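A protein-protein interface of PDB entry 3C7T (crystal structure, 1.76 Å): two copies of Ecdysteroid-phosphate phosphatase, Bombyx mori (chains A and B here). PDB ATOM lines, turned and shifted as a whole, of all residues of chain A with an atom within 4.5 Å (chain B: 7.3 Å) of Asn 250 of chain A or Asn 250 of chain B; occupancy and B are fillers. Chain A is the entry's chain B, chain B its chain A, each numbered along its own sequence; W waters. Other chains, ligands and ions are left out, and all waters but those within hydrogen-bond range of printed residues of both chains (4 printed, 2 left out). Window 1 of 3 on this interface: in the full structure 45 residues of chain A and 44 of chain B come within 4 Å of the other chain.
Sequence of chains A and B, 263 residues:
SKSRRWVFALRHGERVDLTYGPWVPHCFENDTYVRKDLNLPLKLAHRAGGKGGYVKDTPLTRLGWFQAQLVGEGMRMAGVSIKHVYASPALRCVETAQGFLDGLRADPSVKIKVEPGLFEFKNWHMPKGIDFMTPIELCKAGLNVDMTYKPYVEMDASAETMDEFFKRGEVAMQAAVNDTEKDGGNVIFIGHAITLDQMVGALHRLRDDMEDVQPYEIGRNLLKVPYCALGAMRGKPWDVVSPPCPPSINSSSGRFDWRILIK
OE2 of Glu 14 of chain B is in hydrogen-bond range of OG of Ser 251 of chain A, 2.6 Å away.
The side-chain carboxylate (OD2) of Asp 37 of chain B sits at hydrogen-bond distance from the backbone NH (N) of Ile 249 of chain A.
ND2 of Asn 39 of chain B is in hydrogen-bond range of O of Ile 249 of chain A (2.8 Å).
OG of Ser 253 of chain A sits at hydrogen-bond distance from N of Tyr 227 of chain B, 3.3 Å away.
ND2 of Asn 39 of chain A lies within hydrogen-bond range of O of Ile 249 of chain B, at 2.9 Å.
The side-chain amide nitrogen (ND2) of Asn 250 of chain B sits at hydrogen-bond distance from the backbone carbonyl oxygen (O) of Ser 251 of chain A, at 2.9 Å.
O of Asn 250 of chain B lies within hydrogen-bond range of N of Ser 253 of chain A (2.9 Å).
The side-chain hydroxyl (OG) of Ser 251 of chain B sits at hydrogen-bond distance from the side-chain carboxylate (OE2) of Glu 14 of chain A.
The backbone carbonyl oxygen (O) of Ser 251 of chain B is in hydrogen-bond range of the side-chain amide nitrogen (ND2) of Asn 250 of chain A (3.0 Å).
The backbone NH (N) of Asn 250 of chain A is in hydrogen-bond range of the backbone carbonyl oxygen (O) of Ser 253 of chain B (2.9 Å).
O of Ser 251 of chain A lies close to O of Ser 251 of chain B (3.3 Å).
Of the 18 printed residues of chain B, 13 touch a printed residue of chain A.
Printed residues of chain B that touch a printed residue of chain A: Glu 14, Tyr 20, Asp 37, Asn 39, Leu 63, Gln 67, Tyr 227, Ser 248, Ile 249, Asn 250, Ser 251, Ser 252 and Ser 253.
Along chain A the printed residues that touch a printed residue of chain B span positions 14 to 253.
Among the printed residues, no Asp or Glu carboxylate lies within 4 Å of a Lys or Arg side-chain nitrogen of the other chain.
Water W4 bridges OG of Ser 253 of chain A (2.6 Å) and O of Ser 248 of chain B (2.7 Å).
Water W3 lies within hydrogen-bond range of OH of Tyr 227 of chain B (2.7 Å), OG of Ser 251 of chain A (2.8 Å) and OG1 of Thr 19 of chain B (3.1 Å).
Water W2 bridges OG of Ser 251 of chain B (2.7 Å) and OG1 of Thr 19 of chain A (3.2 Å).
Water W1 bridges the side-chain hydroxyl of Ser 253 of chain A (2.9 Å) and the backbone NH of Tyr 227 of chain B (3.0 Å).
Leu 63 of chain A touches Asn 250 of chain B, and with the chains exchanged Asn 250 of chain A touches Leu 63 of chain B.
Asn 250 of chain A touches Ser 251 of chain B, and with the chains exchanged Ser 251 of chain A touches Asn 250 of chain B.
Asn 250 of chain A touches Ser 252 of chain B, and with the chains exchanged Ser 252 of chain A touches Asn 250 of chain B.
Ser 251 of chain A touches its own counterpart, Ser 251 of chain B.
Of the 32 pairs that touch across the chains among the printed residues, 26 have their exchanged pair printed and touching as well.
The side-chain carboxylate of Glu 14 of chain B sits at hydrogen-bond distance from the side-chain amide nitrogen of Asn 39 of chain B.
OE1 of Glu 14 of chain B is in hydrogen-bond range of OG1 of Thr 61 of chain B, at 2.6 Å.
NE of Arg 255 of chain B lies within salt-bridge range of OD1 of Asp 37 of chain B (2.9 Å).
The side-chain carboxylate of Glu 14 of chain A lies within hydrogen-bond range of the side-chain amide nitrogen of Asn 39 of chain A.
The side-chain amide oxygen (OD1) of Asn 39 of chain A is in hydrogen-bond range of the backbone NH (N) of Leu 63 of chain A (2.8 Å).
OD1 of Asn 250 of chain A sits at hydrogen-bond distance from NE2 of Gln 67 of chain A, at 3.1 Å.
Among the printed residues, pairs that only touch across the chains: Glu 14 of chain A with Asn 250 of chain B, Thr 19 of chain A with Ile 249 of chain B, Asn 39 of chain A with Ser 248 of chain B, Asn 39 of chain A with Asn 250 of chain B, Leu 63 of chain A with Leu 63 of chain B, Leu 63 of chain A with Asn 250 of chain B, Gln 67 of chain A with Ser 253 of chain B, Ile 249 of chain A with Tyr 20 of chain B, Ile 249 of chain A with Ser 253 of chain B, Asn 250 of chain A with Glu 14 of chain B, Asn 250 of chain A with Asn 39 of chain B, Asn 250 of chain A with Leu 63 of chain B, Asn 250 of chain A with Asn 250 of chain B, Asn 250 of chain A with Ser 252 of chain B, Ser 251 of chain A with Tyr 227 of chain B, Ser 251 of chain A with Ser 252 of chain B, Ser 252 of chain A with Asn 250 of chain B, Ser 252 of chain A with Ser 251 of chain B, Ser 252 of chain A with Ser 252 of chain B, Ser 253 of chain A with Gln 67 of chain B and Ser 253 of chain A with Ile 249 of chain B.
Printed residues of chain B within 4 Å of Ile 249 of chain A: Tyr 20, Asp 37, Asn 39 and Ser 253.
Printed residues of chain B within 4 Å of Asn 250 of chain A: Glu 14 (3.8 Å), Asn 39 (3.6 Å), Leu 63 (3.6 Å), Asn 250 (3.998 Å), Ser 251 (3.0 Å), Ser 252 (3.4 Å) and Ser 253 (2.9 Å).
Of the printed residues of chain A, Glu 14 of chain B touches Asn 250 and Ser 251.
Printed residues of chain A within 4 Å of Asn 250 of chain B: Glu 14 (3.9 Å), Asn 39 (3.6 Å), Leu 63 (3.7 Å), Asn 250 (3.998 Å), Ser 251 (2.9 Å), Ser 252 (3.4 Å) and Ser 253 (2.9 Å).
Gly 254 of chain B touches none of the printed residues of chain A.
The nearest printed residue of chain B that does not touch Asn 250 of chain A is Thr 19 of chain B (4.3 Å).
The nearest printed residue of chain A that does not touch Asn 250 of chain B is Thr 19 of chain A (4.2 Å).
The nearest printed residue of chain A that does not touch Tyr 20 of chain B is Asn 250 of chain A (5.8 Å).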
ATOM      1  N   GLU A  14      25.964   2.858  17.383  1.00  0.00           N
ATOM      2  CA  GLU A  14      24.580   2.738  16.958  1.00  0.00           C
ATOM      3  C   GLU A  14      23.671   3.719  17.705  1.00  0.00           C
ATOM      4  O   GLU A  14      23.739   3.832  18.928  1.00  0.00           O
ATOM      5  CB  GLU A  14      24.122   1.292  17.208  1.00  0.00           C
ATOM      6  CG  GLU A  14      22.669   1.044  16.840  1.00  0.00           C
ATOM      7  CD  GLU A  14      22.222  -0.385  17.137  1.00  0.00           C
ATOM      8  OE1 GLU A  14      21.969  -0.708  18.306  1.00  0.00           O
ATOM      9  OE2 GLU A  14      22.103  -1.184  16.169  1.00  0.00           O
ATOM     10  N   THR A  19      17.539   3.184  15.156  1.00  0.00           N
ATOM     11  CA  THR A  19      17.245   1.792  15.485  1.00  0.00           C
ATOM     12  C   THR A  19      15.772   1.564  15.838  1.00  0.00           C
ATOM     13  O   THR A  19      15.236   0.456  15.600  1.00  0.00           O
ATOM     14  CB  THR A  19      18.151   1.343  16.665  1.00  0.00           C
ATOM     15  OG1 THR A  19      19.519   1.582  16.317  1.00  0.00           O
ATOM     16  CG2 THR A  19      17.973  -0.142  17.000  1.00  0.00           C
ATOM     17  N   ASN A  39      17.685  -3.041  24.336  1.00  0.00           N
ATOM     18  CA  ASN A  39      18.737  -2.266  23.656  1.00  0.00           C
ATOM     19  C   ASN A  39      18.590  -0.735  23.856  1.00  0.00           C
ATOM     20  O   ASN A  39      19.401   0.073  23.394  1.00  0.00           O
ATOM     21  CB  ASN A  39      18.860  -2.736  22.181  1.00  0.00           C
ATOM     22  CG  ASN A  39      20.145  -2.255  21.516  1.00  0.00           C
ATOM     23  OD1 ASN A  39      21.177  -2.154  22.169  1.00  0.00           O
ATOM     24  ND2 ASN A  39      20.065  -1.926  20.224  1.00  0.00           N
ATOM     25  N   LEU A  63      23.918  -1.455  22.400  1.00  0.00           N
ATOM     26  CA  LEU A  63      24.900  -1.948  21.474  1.00  0.00           C
ATOM     27  C   LEU A  63      25.880  -0.841  21.053  1.00  0.00           C
ATOM     28  O   LEU A  63      27.056  -1.118  20.856  1.00  0.00           O
ATOM     29  CB  LEU A  63      24.216  -2.599  20.261  1.00  0.00           C
ATOM     30  CG  LEU A  63      25.128  -2.926  19.090  1.00  0.00           C
ATOM     31  CD1 LEU A  63      26.255  -3.912  19.512  1.00  0.00           C
ATOM     32  CD2 LEU A  63      24.249  -3.477  17.973  1.00  0.00           C
ATOM     33  N   GLN A  67      29.788  -1.435  21.047  1.00  0.00           N
ATOM     34  CA  GLN A  67      30.645  -1.151  19.889  1.00  0.00           C
ATOM     35  C   GLN A  67      31.833  -0.251  20.243  1.00  0.00           C
ATOM     36  O   GLN A  67      32.992  -0.544  19.899  1.00  0.00           O
ATOM     37  CB  GLN A  67      29.804  -0.492  18.778  1.00  0.00           C
ATOM     38  CG  GLN A  67      28.836  -1.465  18.102  1.00  0.00           C
ATOM     39  CD  GLN A  67      27.833  -0.790  17.210  1.00  0.00           C
ATOM     40  OE1 GLN A  67      27.529   0.407  17.375  1.00  0.00           O
ATOM     41  NE2 GLN A  67      27.256  -1.569  16.273  1.00  0.00           N
ATOM     42  N   ILE A 249      32.044  -6.123  12.566  1.00  0.00           N
ATOM     43  CA  ILE A 249      30.776  -6.317  11.855  1.00  0.00           C
ATOM     44  C   ILE A 249      29.796  -7.031  12.795  1.00  0.00           C
ATOM     45  O   ILE A 249      30.173  -7.974  13.493  1.00  0.00           O
ATOM     46  CB  ILE A 249      30.929  -7.148  10.524  1.00  0.00           C
ATOM     47  CG1 ILE A 249      29.549  -7.491   9.929  1.00  0.00           C
ATOM     48  CG2 ILE A 249      31.670  -8.465  10.782  1.00  0.00           C
ATOM     49  CD1 ILE A 249      29.588  -7.926   8.474  1.00  0.00           C
ATOM     50  N   ASN A 250      28.544  -6.585  12.812  1.00  0.00           N
ATOM     51  CA  ASN A 250      27.483  -7.335  13.485  1.00  0.00           C
ATOM     52  C   ASN A 250      26.239  -7.342  12.633  1.00  0.00           C
ATOM     53  O   ASN A 250      26.040  -6.480  11.747  1.00  0.00           O
ATOM     54  CB  ASN A 250      27.212  -6.803  14.909  1.00  0.00           C
ATOM     55  CG  ASN A 250      26.667  -5.376  14.936  1.00  0.00           C
ATOM     56  OD1 ASN A 250      27.407  -4.406  15.163  1.00  0.00           O
ATOM     57  ND2 ASN A 250      25.380  -5.247  14.747  1.00  0.00           N
ATOM     58  N   SER A 251      25.390  -8.320  12.895  1.00  0.00           N
ATOM     59  CA  SER A 251      24.152  -8.395  12.162  1.00  0.00           C
ATOM     60  C   SER A 251      23.010  -7.776  12.961  1.00  0.00           C
ATOM     61  O   SER A 251      23.190  -7.323  14.117  1.00  0.00           O
ATOM     62  CB  SER A 251      23.873  -9.861  11.787  1.00  0.00           C
ATOM     63  OG  SER A 251      23.453 -10.578  12.941  1.00  0.00           O
ATOM     64  N   SER A 252      21.829  -7.727  12.354  1.00  0.00           N
ATOM     65  CA  SER A 252      20.656  -7.222  13.057  1.00  0.00           C
ATOM     66  C   SER A 252      19.918  -8.312  13.862  1.00  0.00           C
ATOM     67  O   SER A 252      20.158  -9.515  13.713  1.00  0.00           O
ATOM     68  CB  SER A 252      19.707  -6.556  12.063  1.00  0.00           C
ATOM     69  OG  SER A 252      19.306  -7.512  11.085  1.00  0.00           O
ATOM     70  N   SER A 253      18.990  -7.890  14.705  1.00  0.00           N
ATOM     71  CA  SER A 253      18.122  -8.840  15.368  1.00  0.00           C
ATOM     72  C   SER A 253      16.841  -8.110  15.695  1.00  0.00           C
ATOM     73  O   SER A 253      16.867  -7.083  16.377  1.00  0.00           O
ATOM     74  CB  SER A 253      18.791  -9.384  16.638  1.00  0.00           C
ATOM     75  OG  SER A 253      17.953 -10.356  17.270  1.00  0.00           O
ATOM     76  N   GLU B  14      23.567 -14.199  18.755  1.00  0.00           N
ATOM     77  CA  GLU B  14      24.127 -14.078  17.394  1.00  0.00           C
ATOM     78  C   GLU B  14      25.258 -15.070  17.131  1.00  0.00           C
ATOM     79  O   GLU B  14      26.187 -15.179  17.930  1.00  0.00           O
ATOM     80  CB  GLU B  14      24.654 -12.647  17.187  1.00  0.00           C
ATOM     81  CG  GLU B  14      25.272 -12.396  15.810  1.00  0.00           C
ATOM     82  CD  GLU B  14      25.756 -10.968  15.624  1.00  0.00           C
ATOM     83  OE1 GLU B  14      26.831 -10.596  16.164  1.00  0.00           O
ATOM     84  OE2 GLU B  14      25.064 -10.221  14.896  1.00  0.00           O
ATOM     85  N   THR B  19      27.075 -14.618  10.757  1.00  0.00           N
ATOM     86  CA  THR B  19      27.485 -13.219  10.689  1.00  0.00           C
ATOM     87  C   THR B  19      28.648 -13.001   9.734  1.00  0.00           C
ATOM     88  O   THR B  19      28.761 -11.927   9.138  1.00  0.00           O
ATOM     89  CB  THR B  19      27.896 -12.735  12.108  1.00  0.00           C
ATOM     90  OG1 THR B  19      26.780 -12.904  12.982  1.00  0.00           O
ATOM     91  CG2 THR B  19      28.347 -11.267  12.114  1.00  0.00           C
ATOM     92  N   TYR B  20      29.498 -14.025   9.597  1.00  0.00           N
ATOM     93  CA  TYR B  20      30.686 -13.973   8.745  1.00  0.00           C
ATOM     94  C   TYR B  20      30.622 -15.008   7.631  1.00  0.00           C
ATOM     95  O   TYR B  20      29.717 -15.802   7.579  1.00  0.00           O
ATOM     96  CB  TYR B  20      31.938 -14.252   9.580  1.00  0.00           C
ATOM     97  CG  TYR B  20      32.134 -13.252  10.713  1.00  0.00           C
ATOM     98  CD1 TYR B  20      31.474 -13.417  11.932  1.00  0.00           C
ATOM     99  CD2 TYR B  20      32.971 -12.146  10.550  1.00  0.00           C
ATOM    100  CE1 TYR B  20      31.641 -12.486  12.993  1.00  0.00           C
ATOM    101  CE2 TYR B  20      33.143 -11.216  11.606  1.00  0.00           C
ATOM    102  CZ  TYR B  20      32.481 -11.400  12.805  1.00  0.00           C
ATOM    103  OH  TYR B  20      32.666 -10.480  13.836  1.00  0.00           O
ATOM    104  N   ASP B  37      38.453  -9.647  13.690  1.00  0.00           N
ATOM    105  CA  ASP B  37      37.312  -8.732  13.745  1.00  0.00           C
ATOM    106  C   ASP B  37      36.956  -8.525  15.199  1.00  0.00           C
ATOM    107  O   ASP B  37      37.063  -9.462  15.988  1.00  0.00           O
ATOM    108  CB  ASP B  37      36.110  -9.346  13.008  1.00  0.00           C
ATOM    109  CG  ASP B  37      34.975  -8.322  12.774  1.00  0.00           C
ATOM    110  OD1 ASP B  37      35.062  -7.550  11.802  1.00  0.00           O
ATOM    111  OD2 ASP B  37      33.997  -8.317  13.554  1.00  0.00           O
ATOM    112  N   ASN B  39      34.108  -8.256  16.591  1.00  0.00           N
ATOM    113  CA  ASN B  39      32.954  -9.025  16.999  1.00  0.00           C
ATOM    114  C   ASN B  39      33.235 -10.547  16.989  1.00  0.00           C
ATOM    115  O   ASN B  39      32.354 -11.357  17.280  1.00  0.00           O
ATOM    116  CB  ASN B  39      31.746  -8.631  16.112  1.00  0.00           C
ATOM    117  CG  ASN B  39      30.426  -9.105  16.659  1.00  0.00           C
ATOM    118  OD1 ASN B  39      30.218  -9.156  17.876  1.00  0.00           O
ATOM    119  ND2 ASN B  39      29.500  -9.439  15.749  1.00  0.00           N
ATOM    120  N   THR B  61      29.157 -14.686  18.550  1.00  0.00           N
ATOM    121  CA  THR B  61      29.923 -13.450  18.359  1.00  0.00           C
ATOM    122  C   THR B  61      29.998 -12.749  19.723  1.00  0.00           C
ATOM    123  O   THR B  61      29.297 -13.153  20.673  1.00  0.00           O
ATOM    124  CB  THR B  61      29.196 -12.510  17.394  1.00  0.00           C
ATOM    125  OG1 THR B  61      27.891 -12.244  17.898  1.00  0.00           O
ATOM    126  CG2 THR B  61      29.095 -13.188  16.001  1.00  0.00           C
ATOM    127  N   LEU B  63      28.746  -9.859  20.201  1.00  0.00           N
ATOM    128  CA  LEU B  63      27.397  -9.328  20.333  1.00  0.00           C
ATOM    129  C   LEU B  63      26.480 -10.423  20.886  1.00  0.00           C
ATOM    130  O   LEU B  63      25.600 -10.153  21.682  1.00  0.00           O
ATOM    131  CB  LEU B  63      26.867  -8.860  18.983  1.00  0.00           C
ATOM    132  CG  LEU B  63      25.433  -8.340  18.992  1.00  0.00           C
ATOM    133  CD1 LEU B  63      25.167  -7.393  20.189  1.00  0.00           C
ATOM    134  CD2 LEU B  63      25.100  -7.700  17.663  1.00  0.00           C
ATOM    135  N   GLN B  67      24.010  -9.910  23.934  1.00  0.00           N
ATOM    136  CA  GLN B  67      22.556 -10.165  23.889  1.00  0.00           C
ATOM    137  C   GLN B  67      22.087 -11.061  25.022  1.00  0.00           C
ATOM    138  O   GLN B  67      21.072 -10.768  25.668  1.00  0.00           O
ATOM    139  CB  GLN B  67      22.175 -10.808  22.540  1.00  0.00           C
ATOM    140  CG  GLN B  67      22.390  -9.852  21.361  1.00  0.00           C
ATOM    141  CD  GLN B  67      22.247 -10.519  19.970  1.00  0.00           C
ATOM    142  OE1 GLN B  67      22.464 -11.736  19.817  1.00  0.00           O
ATOM    143  NE2 GLN B  67      21.946  -9.699  18.926  1.00  0.00           N
ATOM    144  N   LEU B  70      22.276  -9.153  28.332  1.00  0.00           N
ATOM    145  CA  LEU B  70      21.178  -8.213  28.475  1.00  0.00           C
ATOM    146  C   LEU B  70      19.910  -8.873  28.997  1.00  0.00           C
ATOM    147  O   LEU B  70      19.170  -8.268  29.821  1.00  0.00           O
ATOM    148  CB  LEU B  70      20.885  -7.529  27.146  1.00  0.00           C
ATOM    149  CG  LEU B  70      21.938  -6.518  26.736  1.00  0.00           C
ATOM    150  CD1 LEU B  70      21.564  -6.077  25.307  1.00  0.00           C
ATOM    151  CD2 LEU B  70      22.004  -5.329  27.719  1.00  0.00           C
ATOM    152  N   TYR B 227      17.313 -13.586  17.696  1.00  0.00           N
ATOM    153  CA  TYR B 227      18.354 -14.036  18.621  1.00  0.00           C
ATOM    154  C   TYR B 227      17.999 -13.635  20.038  1.00  0.00           C
ATOM    155  O   TYR B 227      17.528 -12.505  20.265  1.00  0.00           O
ATOM    156  CB  TYR B 227      19.665 -13.377  18.258  1.00  0.00           C
ATOM    157  CG  TYR B 227      20.344 -13.850  16.984  1.00  0.00           C
ATOM    158  CD1 TYR B 227      20.575 -15.215  16.749  1.00  0.00           C
ATOM    159  CD2 TYR B 227      20.864 -12.926  16.076  1.00  0.00           C
ATOM    160  CE1 TYR B 227      21.264 -15.635  15.617  1.00  0.00           C
ATOM    161  CE2 TYR B 227      21.559 -13.338  14.925  1.00  0.00           C
ATOM    162  CZ  TYR B 227      21.748 -14.706  14.708  1.00  0.00           C
ATOM    163  OH  TYR B 227      22.449 -15.140  13.602  1.00  0.00           O
ATOM    164  N   SER B 248      14.055  -7.205  22.694  1.00  0.00           N
ATOM    165  CA  SER B 248      15.218  -6.425  22.241  1.00  0.00           C
ATOM    166  C   SER B 248      15.256  -6.296  20.721  1.00  0.00           C
ATOM    167  O   SER B 248      14.810  -7.214  20.016  1.00  0.00           O
ATOM    168  CB  SER B 248      16.497  -7.132  22.713  1.00  0.00           C
ATOM    169  OG  SER B 248      17.621  -6.291  22.533  1.00  0.00           O
ATOM    170  N   ILE B 249      15.844  -5.210  20.215  1.00  0.00           N
ATOM    171  CA  ILE B 249      16.132  -5.081  18.793  1.00  0.00           C
ATOM    172  C   ILE B 249      17.456  -4.365  18.607  1.00  0.00           C
ATOM    173  O   ILE B 249      17.742  -3.375  19.286  1.00  0.00           O
ATOM    174  CB  ILE B 249      15.017  -4.280  18.016  1.00  0.00           C
ATOM    175  CG1 ILE B 249      15.347  -4.200  16.531  1.00  0.00           C
ATOM    176  CG2 ILE B 249      14.747  -2.911  18.663  1.00  0.00           C
ATOM    177  CD1 ILE B 249      14.336  -3.421  15.694  1.00  0.00           C
ATOM    178  N   ASN B 250      18.258  -4.842  17.663  1.00  0.00           N
ATOM    179  CA  ASN B 250      19.438  -4.071  17.241  1.00  0.00           C
ATOM    180  C   ASN B 250      19.575  -4.083  15.727  1.00  0.00           C
ATOM    181  O   ASN B 250      19.044  -4.980  15.052  1.00  0.00           O
ATOM    182  CB  ASN B 250      20.737  -4.550  17.909  1.00  0.00           C
ATOM    183  CG  ASN B 250      21.113  -5.951  17.524  1.00  0.00           C
ATOM    184  OD1 ASN B 250      20.732  -6.909  18.219  1.00  0.00           O
ATOM    185  ND2 ASN B 250      21.849  -6.103  16.416  1.00  0.00           N
ATOM    186  N   SER B 251      20.274  -3.083  15.203  1.00  0.00           N
ATOM    187  CA  SER B 251      20.509  -3.001  13.773  1.00  0.00           C
ATOM    188  C   SER B 251      21.863  -3.621  13.424  1.00  0.00           C
ATOM    189  O   SER B 251      22.625  -4.049  14.312  1.00  0.00           O
ATOM    190  CB  SER B 251      20.441  -1.549  13.296  1.00  0.00           C
ATOM    191  OG  SER B 251      21.542  -0.802  13.776  1.00  0.00           O
ATOM    192  N   SER B 252      22.161  -3.697  12.133  1.00  0.00           N
ATOM    193  CA  SER B 252      23.425  -4.249  11.668  1.00  0.00           C
ATOM    194  C   SER B 252      24.499  -3.138  11.607  1.00  0.00           C
ATOM    195  O   SER B 252      24.189  -1.927  11.709  1.00  0.00           O
ATOM    196  CB  SER B 252      23.223  -4.802  10.245  1.00  0.00           C
ATOM    197  OG  SER B 252      22.898  -3.720   9.369  1.00  0.00           O
ATOM    198  N   SER B 253      25.751  -3.538  11.422  1.00  0.00           N
ATOM    199  CA  SER B 253      26.819  -2.598  11.178  1.00  0.00           C
ATOM    200  C   SER B 253      27.888  -3.354  10.414  1.00  0.00           C
ATOM    201  O   SER B 253      28.359  -4.419  10.873  1.00  0.00           O
ATOM    202  CB  SER B 253      27.382  -2.013  12.497  1.00  0.00           C
ATOM    203  OG  SER B 253      28.343  -0.985  12.189  1.00  0.00           O
ATOM    204  N   GLY B 254      28.257  -2.804   9.260  1.00  0.00           N
ATOM    205  CA  GLY B 254      29.221  -3.421   8.387  1.00  0.00           C
ATOM    206  C   GLY B 254      30.654  -3.177   8.798  1.00  0.00           C
ATOM    207  O   GLY B 254      30.940  -2.469   9.783  1.00  0.00           O
ATOM    208  N   ARG B 255      31.556  -3.780   8.030  1.00  0.00           N
ATOM    209  CA  ARG B 255      32.967  -3.795   8.363  1.00  0.00           C
ATOM    210  C   ARG B 255      33.696  -2.662   7.612  1.00  0.00           C
ATOM    211  O   ARG B 255      33.611  -2.566   6.387  1.00  0.00           O
ATOM    212  CB  ARG B 255      33.522  -5.182   8.006  1.00  0.00           C
ATOM    213  CG  ARG B 255      34.765  -5.583   8.701  1.00  0.00           C
ATOM    214  CD  ARG B 255      34.964  -7.117   8.590  1.00  0.00           C
ATOM    215  NE  ARG B 255      36.250  -7.557   9.136  1.00  0.00           N
ATOM    216  CZ  ARG B 255      37.374  -7.669   8.432  1.00  0.00           C
ATOM    217  NH1 ARG B 255      37.392  -7.375   7.142  1.00  0.00           N
ATOM    218  NH2 ARG B 255      38.491  -8.075   9.015  1.00  0.00           N
HETATM  219  O   HOH W   1      17.498 -12.223  15.040  1.00  0.00           O
HETATM  220  O   HOH W   2      20.808   1.817  13.446  1.00  0.00           O
HETATM  221  O   HOH W   3      23.802 -13.240  12.208  1.00  0.00           O
HETATM  222  O   HOH W   4      16.592  -9.011  19.058  1.00  0.00           O
